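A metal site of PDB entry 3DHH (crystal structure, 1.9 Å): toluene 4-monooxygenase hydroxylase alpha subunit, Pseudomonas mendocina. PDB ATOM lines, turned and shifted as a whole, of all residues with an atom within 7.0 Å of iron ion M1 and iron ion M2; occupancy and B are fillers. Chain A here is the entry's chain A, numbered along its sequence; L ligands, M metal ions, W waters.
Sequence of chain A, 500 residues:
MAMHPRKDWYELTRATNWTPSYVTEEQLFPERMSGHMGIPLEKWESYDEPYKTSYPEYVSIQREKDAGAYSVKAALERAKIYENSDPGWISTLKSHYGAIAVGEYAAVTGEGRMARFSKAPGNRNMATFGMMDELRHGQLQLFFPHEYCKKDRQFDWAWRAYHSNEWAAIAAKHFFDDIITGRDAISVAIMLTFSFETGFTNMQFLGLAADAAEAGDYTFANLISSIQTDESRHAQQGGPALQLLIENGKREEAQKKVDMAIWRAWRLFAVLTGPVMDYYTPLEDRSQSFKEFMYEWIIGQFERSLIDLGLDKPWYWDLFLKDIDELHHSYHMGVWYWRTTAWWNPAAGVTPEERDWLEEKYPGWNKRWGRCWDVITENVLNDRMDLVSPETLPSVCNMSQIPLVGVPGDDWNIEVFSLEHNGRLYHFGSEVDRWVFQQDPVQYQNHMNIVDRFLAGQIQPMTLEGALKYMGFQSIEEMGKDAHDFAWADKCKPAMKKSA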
ATOM      1  N   ILE A 100      -6.022  17.676  -7.696  1.00  0.00           N
ATOM      2  CA  ILE A 100      -6.105  19.101  -8.085  1.00  0.00           C
ATOM      3  C   ILE A 100      -4.825  19.925  -8.041  1.00  0.00           C
ATOM      4  O   ILE A 100      -4.564  20.664  -8.985  1.00  0.00           O
ATOM      5  CB  ILE A 100      -7.232  19.832  -7.281  1.00  0.00           C
ATOM      6  CG1 ILE A 100      -8.603  19.308  -7.703  1.00  0.00           C
ATOM      7  CG2 ILE A 100      -7.150  21.360  -7.409  1.00  0.00           C
ATOM      8  CD1 ILE A 100      -8.894  19.312  -9.207  1.00  0.00           C
ATOM      9  N   GLY A 103      -2.376  19.839 -10.924  1.00  0.00           N
ATOM     10  CA  GLY A 103      -3.172  20.220 -12.117  1.00  0.00           C
ATOM     11  C   GLY A 103      -3.394  21.734 -12.240  1.00  0.00           C
ATOM     12  O   GLY A 103      -3.273  22.269 -13.328  1.00  0.00           O
ATOM     13  N   GLU A 104      -3.696  22.408 -11.123  1.00  0.00           N
ATOM     14  CA  GLU A 104      -3.708  23.879 -11.077  1.00  0.00           C
ATOM     15  C   GLU A 104      -2.391  24.425 -11.591  1.00  0.00           C
ATOM     16  O   GLU A 104      -2.355  25.297 -12.448  1.00  0.00           O
ATOM     17  CB  GLU A 104      -3.889  24.349  -9.613  1.00  0.00           C
ATOM     18  CG  GLU A 104      -5.230  23.919  -9.036  1.00  0.00           C
ATOM     19  CD  GLU A 104      -6.338  24.924  -9.270  1.00  0.00           C
ATOM     20  OE1 GLU A 104      -7.363  24.873  -8.566  1.00  0.00           O
ATOM     21  OE2 GLU A 104      -6.207  25.749 -10.169  1.00  0.00           O
ATOM     22  N   TYR A 105      -1.274  23.918 -11.076  1.00  0.00           N
ATOM     23  CA  TYR A 105       0.012  24.375 -11.571  1.00  0.00           C
ATOM     24  C   TYR A 105       0.242  24.094 -13.091  1.00  0.00           C
ATOM     25  O   TYR A 105       0.776  24.942 -13.797  1.00  0.00           O
ATOM     26  CB  TYR A 105       1.161  23.810 -10.697  1.00  0.00           C
ATOM     27  CG  TYR A 105       2.467  24.460 -11.051  1.00  0.00           C
ATOM     28  CD1 TYR A 105       2.761  25.737 -10.599  1.00  0.00           C
ATOM     29  CD2 TYR A 105       3.355  23.834 -11.916  1.00  0.00           C
ATOM     30  CE1 TYR A 105       3.959  26.365 -10.960  1.00  0.00           C
ATOM     31  CE2 TYR A 105       4.568  24.449 -12.283  1.00  0.00           C
ATOM     32  CZ  TYR A 105       4.838  25.723 -11.818  1.00  0.00           C
ATOM     33  OH  TYR A 105       5.997  26.367 -12.173  1.00  0.00           O
ATOM     34  N   ALA A 107      -2.162  24.184 -15.200  1.00  0.00           N
ATOM     35  CA  ALA A 107      -2.988  25.231 -15.842  1.00  0.00           C
ATOM     36  C   ALA A 107      -2.241  26.565 -16.076  1.00  0.00           C
ATOM     37  O   ALA A 107      -2.626  27.338 -16.967  1.00  0.00           O
ATOM     38  CB  ALA A 107      -4.296  25.445 -15.076  1.00  0.00           C
ATOM     39  N   GLU A 111      -2.511  28.879 -19.643  1.00  0.00           N
ATOM     40  CA  GLU A 111      -2.621  30.339 -19.646  1.00  0.00           C
ATOM     41  C   GLU A 111      -1.389  30.962 -20.300  1.00  0.00           C
ATOM     42  O   GLU A 111      -1.516  31.908 -21.104  1.00  0.00           O
ATOM     43  CB  GLU A 111      -2.819  30.874 -18.230  1.00  0.00           C
ATOM     44  CG  GLU A 111      -4.174  30.471 -17.570  1.00  0.00           C
ATOM     45  CD  GLU A 111      -5.376  31.310 -18.093  1.00  0.00           C
ATOM     46  OE1 GLU A 111      -5.165  32.347 -18.737  1.00  0.00           O
ATOM     47  OE2 GLU A 111      -6.546  30.935 -17.844  1.00  0.00           O
ATOM     48  N   GLY A 130      -4.286  35.245 -15.664  1.00  0.00           N
ATOM     49  CA  GLY A 130      -4.647  33.825 -15.496  1.00  0.00           C
ATOM     50  C   GLY A 130      -3.469  32.965 -15.094  1.00  0.00           C
ATOM     51  O   GLY A 130      -3.618  32.045 -14.272  1.00  0.00           O
ATOM     52  N   ASP A 133      -3.083  33.659 -11.405  1.00  0.00           N
ATOM     53  CA  ASP A 133      -4.156  33.009 -10.672  1.00  0.00           C
ATOM     54  C   ASP A 133      -3.860  31.478 -10.459  1.00  0.00           C
ATOM     55  O   ASP A 133      -4.062  30.961  -9.444  1.00  0.00           O
ATOM     56  CB  ASP A 133      -5.472  33.116 -11.429  1.00  0.00           C
ATOM     57  CG  ASP A 133      -6.036  34.520 -11.502  1.00  0.00           C
ATOM     58  OD1 ASP A 133      -5.684  35.392 -10.765  1.00  0.00           O
ATOM     59  OD2 ASP A 133      -6.892  34.702 -12.322  1.00  0.00           O
ATOM     60  N   GLU A 134      -3.376  30.809 -11.480  1.00  0.00           N
ATOM     61  CA  GLU A 134      -3.194  29.382 -11.371  1.00  0.00           C
ATOM     62  C   GLU A 134      -1.976  29.081 -10.531  1.00  0.00           C
ATOM     63  O   GLU A 134      -1.980  28.187  -9.825  1.00  0.00           O
ATOM     64  CB  GLU A 134      -3.170  28.650 -12.710  1.00  0.00           C
ATOM     65  CG  GLU A 134      -4.309  28.919 -13.633  1.00  0.00           C
ATOM     66  CD  GLU A 134      -5.638  28.404 -13.151  1.00  0.00           C
ATOM     67  OE1 GLU A 134      -5.755  28.045 -12.025  1.00  0.00           O
ATOM     68  OE2 GLU A 134      -6.525  28.321 -13.913  1.00  0.00           O
ATOM     69  N   LEU A 135      -0.966  29.921 -10.608  1.00  0.00           N
ATOM     70  CA  LEU A 135       0.133  29.863  -9.663  1.00  0.00           C
ATOM     71  C   LEU A 135      -0.414  29.934  -8.227  1.00  0.00           C
ATOM     72  O   LEU A 135      -0.070  29.161  -7.440  1.00  0.00           O
ATOM     73  CB  LEU A 135       1.120  30.966  -9.896  1.00  0.00           C
ATOM     74  CG  LEU A 135       2.377  30.915  -9.059  1.00  0.00           C
ATOM     75  CD1 LEU A 135       3.171  29.697  -9.287  1.00  0.00           C
ATOM     76  CD2 LEU A 135       3.181  32.097  -9.230  1.00  0.00           C
ATOM     77  N   HIS A 137      -3.355  29.162  -7.142  1.00  0.00           N
ATOM     78  CA  HIS A 137      -4.156  27.980  -6.790  1.00  0.00           C
ATOM     79  C   HIS A 137      -3.286  26.749  -6.542  1.00  0.00           C
ATOM     80  O   HIS A 137      -3.550  25.971  -5.625  1.00  0.00           O
ATOM     81  CB  HIS A 137      -5.132  27.669  -7.902  1.00  0.00           C
ATOM     82  CG  HIS A 137      -6.072  28.808  -8.190  1.00  0.00           C
ATOM     83  ND1 HIS A 137      -6.890  28.849  -9.305  1.00  0.00           N
ATOM     84  CD2 HIS A 137      -6.295  29.952  -7.510  1.00  0.00           C
ATOM     85  CE1 HIS A 137      -7.581  29.978  -9.289  1.00  0.00           C
ATOM     86  NE2 HIS A 137      -7.228  30.670  -8.214  1.00  0.00           N
ATOM     87  N   GLY A 138      -2.256  26.597  -7.376  1.00  0.00           N
ATOM     88  CA  GLY A 138      -1.276  25.515  -7.153  1.00  0.00           C
ATOM     89  C   GLY A 138      -0.589  25.668  -5.815  1.00  0.00           C
ATOM     90  O   GLY A 138      -0.449  24.683  -5.069  1.00  0.00           O
ATOM     91  N   GLN A 141      -2.999  25.050  -2.761  1.00  0.00           N
ATOM     92  CA  GLN A 141      -3.466  23.665  -2.588  1.00  0.00           C
ATOM     93  C   GLN A 141      -2.321  22.687  -2.355  1.00  0.00           C
ATOM     94  O   GLN A 141      -2.564  21.497  -2.196  1.00  0.00           O
ATOM     95  CB  GLN A 141      -4.352  23.255  -3.744  1.00  0.00           C
ATOM     96  CG  GLN A 141      -5.701  23.991  -3.624  1.00  0.00           C
ATOM     97  CD  GLN A 141      -6.562  23.943  -4.862  1.00  0.00           C
ATOM     98  OE1 GLN A 141      -6.169  24.401  -5.969  1.00  0.00           O
ATOM     99  NE2 GLN A 141      -7.751  23.437  -4.685  1.00  0.00           N
ATOM    100  N   LEU A 192     -10.418  24.855 -22.224  1.00  0.00           N
ATOM    101  CA  LEU A 192     -10.144  25.156 -20.816  1.00  0.00           C
ATOM    102  C   LEU A 192     -11.015  26.315 -20.297  1.00  0.00           C
ATOM    103  O   LEU A 192     -11.837  26.100 -19.412  1.00  0.00           O
ATOM    104  CB  LEU A 192      -8.679  25.451 -20.557  1.00  0.00           C
ATOM    105  CG  LEU A 192      -8.337  25.913 -19.131  1.00  0.00           C
ATOM    106  CD1 LEU A 192      -8.711  24.823 -18.071  1.00  0.00           C
ATOM    107  CD2 LEU A 192      -6.826  26.255 -19.075  1.00  0.00           C
ATOM    108  N   THR A 193     -10.826  27.526 -20.786  1.00  0.00           N
ATOM    109  CA  THR A 193     -11.440  28.667 -20.068  1.00  0.00           C
ATOM    110  C   THR A 193     -12.953  28.682 -20.226  1.00  0.00           C
ATOM    111  O   THR A 193     -13.661  28.935 -19.259  1.00  0.00           O
ATOM    112  CB  THR A 193     -10.828  30.038 -20.408  1.00  0.00           C
ATOM    113  OG1 THR A 193     -11.138  30.396 -21.765  1.00  0.00           O
ATOM    114  CG2 THR A 193      -9.324  29.970 -20.260  1.00  0.00           C
ATOM    115  N   PHE A 196     -14.361  23.980 -19.548  1.00  0.00           N
ATOM    116  CA  PHE A 196     -14.040  23.463 -18.228  1.00  0.00           C
ATOM    117  C   PHE A 196     -14.267  24.485 -17.104  1.00  0.00           C
ATOM    118  O   PHE A 196     -14.914  24.141 -16.086  1.00  0.00           O
ATOM    119  CB  PHE A 196     -12.594  22.930 -18.239  1.00  0.00           C
ATOM    120  CG  PHE A 196     -12.231  22.130 -17.023  1.00  0.00           C
ATOM    121  CD1 PHE A 196     -12.815  20.901 -16.755  1.00  0.00           C
ATOM    122  CD2 PHE A 196     -11.263  22.599 -16.149  1.00  0.00           C
ATOM    123  CE1 PHE A 196     -12.449  20.188 -15.623  1.00  0.00           C
ATOM    124  CE2 PHE A 196     -10.882  21.880 -15.036  1.00  0.00           C
ATOM    125  CZ  PHE A 196     -11.458  20.680 -14.777  1.00  0.00           C
ATOM    126  N   GLU A 197     -13.763  25.704 -17.269  1.00  0.00           N
ATOM    127  CA  GLU A 197     -13.714  26.671 -16.168  1.00  0.00           C
ATOM    128  C   GLU A 197     -15.020  27.448 -15.963  1.00  0.00           C
ATOM    129  O   GLU A 197     -15.236  27.967 -14.878  1.00  0.00           O
ATOM    130  CB  GLU A 197     -12.562  27.651 -16.344  1.00  0.00           C
ATOM    131  CG  GLU A 197     -11.179  26.992 -16.301  1.00  0.00           C
ATOM    132  CD  GLU A 197     -10.026  28.025 -16.451  1.00  0.00           C
ATOM    133  OE1 GLU A 197     -10.120  28.914 -17.321  1.00  0.00           O
ATOM    134  OE2 GLU A 197      -9.038  27.963 -15.709  1.00  0.00           O
ATOM    135  N   THR A 201     -15.898  23.345 -13.225  1.00  0.00           N
ATOM    136  CA  THR A 201     -15.121  23.540 -11.965  1.00  0.00           C
ATOM    137  C   THR A 201     -15.999  24.047 -10.835  1.00  0.00           C
ATOM    138  O   THR A 201     -15.703  23.771  -9.666  1.00  0.00           O
ATOM    139  CB  THR A 201     -13.915  24.459 -12.114  1.00  0.00           C
ATOM    140  OG1 THR A 201     -14.346  25.719 -12.589  1.00  0.00           O
ATOM    141  CG2 THR A 201     -12.884  23.865 -13.084  1.00  0.00           C
ATOM    142  N   PHE A 205     -15.479  23.321  -6.784  1.00  0.00           N
ATOM    143  CA  PHE A 205     -15.027  24.426  -6.000  1.00  0.00           C
ATOM    144  C   PHE A 205     -16.162  25.232  -5.318  1.00  0.00           C
ATOM    145  O   PHE A 205     -15.922  26.042  -4.442  1.00  0.00           O
ATOM    146  CB  PHE A 205     -14.174  25.330  -6.840  1.00  0.00           C
ATOM    147  CG  PHE A 205     -12.827  24.786  -7.150  1.00  0.00           C
ATOM    148  CD1 PHE A 205     -12.618  24.015  -8.248  1.00  0.00           C
ATOM    149  CD2 PHE A 205     -11.753  25.049  -6.357  1.00  0.00           C
ATOM    150  CE1 PHE A 205     -11.403  23.492  -8.515  1.00  0.00           C
ATOM    151  CE2 PHE A 205     -10.553  24.516  -6.637  1.00  0.00           C
ATOM    152  CZ  PHE A 205     -10.382  23.767  -7.742  1.00  0.00           C
ATOM    153  N   ILE A 227     -10.677  30.609  -4.272  1.00  0.00           N
ATOM    154  CA  ILE A 227     -10.096  30.142  -5.537  1.00  0.00           C
ATOM    155  C   ILE A 227     -11.075  30.332  -6.728  1.00  0.00           C
ATOM    156  O   ILE A 227     -10.699  30.834  -7.798  1.00  0.00           O
ATOM    157  CB  ILE A 227      -9.655  28.653  -5.408  1.00  0.00           C
ATOM    158  CG1 ILE A 227      -8.362  28.563  -4.572  1.00  0.00           C
ATOM    159  CG2 ILE A 227      -9.428  28.043  -6.828  1.00  0.00           C
ATOM    160  CD1 ILE A 227      -7.894  27.056  -4.192  1.00  0.00           C
ATOM    161  N   GLN A 228     -12.343  29.952  -6.540  1.00  0.00           N
ATOM    162  CA  GLN A 228     -13.302  30.096  -7.643  1.00  0.00           C
ATOM    163  C   GLN A 228     -13.561  31.589  -8.029  1.00  0.00           C
ATOM    164  O   GLN A 228     -13.983  31.864  -9.164  1.00  0.00           O
ATOM    165  CB  GLN A 228     -14.616  29.346  -7.337  1.00  0.00           C
ATOM    166  CG  GLN A 228     -15.389  28.943  -8.612  1.00  0.00           C
ATOM    167  CD  GLN A 228     -14.651  27.915  -9.482  1.00  0.00           C
ATOM    168  OE1 GLN A 228     -13.503  27.578  -9.205  1.00  0.00           O
ATOM    169  NE2 GLN A 228     -15.309  27.432 -10.530  1.00  0.00           N
ATOM    170  N   ASP A 230     -11.251  33.713  -8.593  1.00  0.00           N
ATOM    171  CA  ASP A 230     -10.271  33.920  -9.663  1.00  0.00           C
ATOM    172  C   ASP A 230     -10.722  33.316 -10.975  1.00  0.00           C
ATOM    173  O   ASP A 230     -10.644  33.942 -12.020  1.00  0.00           O
ATOM    174  CB  ASP A 230      -8.903  33.307  -9.299  1.00  0.00           C
ATOM    175  CG  ASP A 230      -8.253  33.946  -8.088  1.00  0.00           C
ATOM    176  OD1 ASP A 230      -8.409  35.173  -7.892  1.00  0.00           O
ATOM    177  OD2 ASP A 230      -7.608  33.191  -7.327  1.00  0.00           O
ATOM    178  N   GLU A 231     -11.207  32.078 -10.896  1.00  0.00           N
ATOM    179  CA  GLU A 231     -11.724  31.328 -12.045  1.00  0.00           C
ATOM    180  C   GLU A 231     -12.806  32.126 -12.741  1.00  0.00           C
ATOM    181  O   GLU A 231     -12.810  32.237 -13.969  1.00  0.00           O
ATOM    182  CB  GLU A 231     -12.301  29.990 -11.547  1.00  0.00           C
ATOM    183  CG  GLU A 231     -12.818  29.073 -12.635  1.00  0.00           C
ATOM    184  CD  GLU A 231     -11.729  28.138 -13.147  1.00  0.00           C
ATOM    185  OE1 GLU A 231     -11.921  26.909 -13.123  1.00  0.00           O
ATOM    186  OE2 GLU A 231     -10.663  28.616 -13.539  1.00  0.00           O
ATOM    187  N   SER A 232     -13.723  32.698 -11.966  1.00  0.00           N
ATOM    188  CA  SER A 232     -14.788  33.523 -12.537  1.00  0.00           C
ATOM    189  C   SER A 232     -14.317  34.668 -13.440  1.00  0.00           C
ATOM    190  O   SER A 232     -14.998  34.954 -14.439  1.00  0.00           O
ATOM    191  CB  SER A 232     -15.739  34.022 -11.469  1.00  0.00           C
ATOM    192  OG  SER A 232     -16.328  32.854 -10.888  1.00  0.00           O
ATOM    193  N   HIS A 234     -10.809  34.715 -14.917  1.00  0.00           N
ATOM    194  CA  HIS A 234      -9.992  34.299 -16.053  1.00  0.00           C
ATOM    195  C   HIS A 234     -10.769  33.367 -16.954  1.00  0.00           C
ATOM    196  O   HIS A 234     -10.423  33.254 -18.128  1.00  0.00           O
ATOM    197  CB  HIS A 234      -8.607  33.744 -15.706  1.00  0.00           C
ATOM    198  CG  HIS A 234      -8.611  32.487 -14.886  1.00  0.00           C
ATOM    199  ND1 HIS A 234      -8.056  32.449 -13.630  1.00  0.00           N
ATOM    200  CD2 HIS A 234      -9.019  31.208 -15.162  1.00  0.00           C
ATOM    201  CE1 HIS A 234      -8.134  31.209 -13.150  1.00  0.00           C
ATOM    202  NE2 HIS A 234      -8.719  30.448 -14.056  1.00  0.00           N
ATOM    203  N   ALA A 235     -11.838  32.735 -16.432  1.00  0.00           N
ATOM    204  CA  ALA A 235     -12.663  31.864 -17.307  1.00  0.00           C
ATOM    205  C   ALA A 235     -13.362  32.660 -18.412  1.00  0.00           C
ATOM    206  O   ALA A 235     -13.746  32.097 -19.433  1.00  0.00           O
ATOM    207  CB  ALA A 235     -13.635  31.030 -16.541  1.00  0.00           C
HETATM  208  O1  LIG L   1      -7.712  25.798 -12.419  1.00  0.00           O
HETATM  209  C1  LIG L   1      -7.887  24.101 -14.069  1.00  0.00           C
HETATM  210  C2  LIG L   1      -8.451  25.430 -13.580  1.00  0.00           C
HETATM  211  O2  LIG L   1      -7.263  23.339 -13.021  1.00  0.00           O
HETATM  212  C3  LIG L   1      -8.121  21.457 -11.862  1.00  0.00           C
HETATM  213  C4  LIG L   1      -8.119  22.958 -11.920  1.00  0.00           C
HETATM  214  O3  LIG L   1      -6.852  20.981 -12.348  1.00  0.00           O
HETATM  215  C5  LIG L   1      -6.427  19.881 -11.575  1.00  0.00           C
HETATM  216 FE    FE M   1      -8.753  28.326 -13.664  1.00  0.00          FE
HETATM  217 FE    FE M   2      -7.359  27.289 -10.877  1.00  0.00          FE
HETATM  218  O   HOH W   1      -9.013  26.428  -9.617  1.00  0.00           O
HETATM  219  O   HOH W   2      -8.857  28.505 -11.772  1.00  0.00           O
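Iron ion M2 is bound by the side-chain carboxylate of Glu 104 (2.0 Å), the side-chain carboxylate of Glu 134 (2.1 Å), water W2 (2.1 Å), an oxygen (O1) of the ligand (2.2 Å), water W1 (2.3 Å) and a ring nitrogen (ND1) of His 137 (2.3 Å). Iron ion M2 has six donor atoms within binding distance.
Iron ion M1 is bound by water W2 (1.9 Å), OE2 of Glu 231 (1.9 Å), OE2 of Glu 197 (2.1 Å), NE2 of His 234 (2.2 Å) and OE2 of Glu 134 (2.2 Å). Iron ion M1 has five donor atoms within binding distance.
The side-chain carboxylate (OE1) of Glu 104 sits close to the side-chain amide oxygen (OE1) of Gln 141 (2.9 Å). The backbone carbonyl oxygen (O) of Leu 192 lies within hydrogen-bond range of the backbone NH (N) of Glu 197 (2.9 Å). The backbone carbonyl oxygen (O) of Glu 197 is in hydrogen-bond range of the side-chain hydroxyl (OG1) of Thr 201 (3.3 Å). A ring nitrogen (ND1) of His 234 sits at hydrogen-bond distance from the side-chain carboxylate of Asp 133 (2.9 Å). ND1 of His 234 sits at hydrogen-bond distance from O of Asp 230, at 3.4 Å. O of Ile 227 sits at hydrogen-bond distance from NE2 of His 137 (3.5 Å). The side-chain amide oxygen of Gln 141 lies close to the backbone carbonyl oxygen of His 137 (3.1 Å). The side-chain carboxylate (OD2) of Asp 230 sits at hydrogen-bond distance from a ring nitrogen (NE2) of His 137 (2.7 Å).
Of the 26 residues printed, 3 come within 4 Å of iron ion M2. The nearest printed residue that does not touch iron ion M2 is Glu 231 (4.4 Å).
Along chain A the residues within 4 Å of iron ion M1 span positions 134 to 234. The nearest printed residue that does not touch iron ion M1 is His 137 (4.8 Å).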
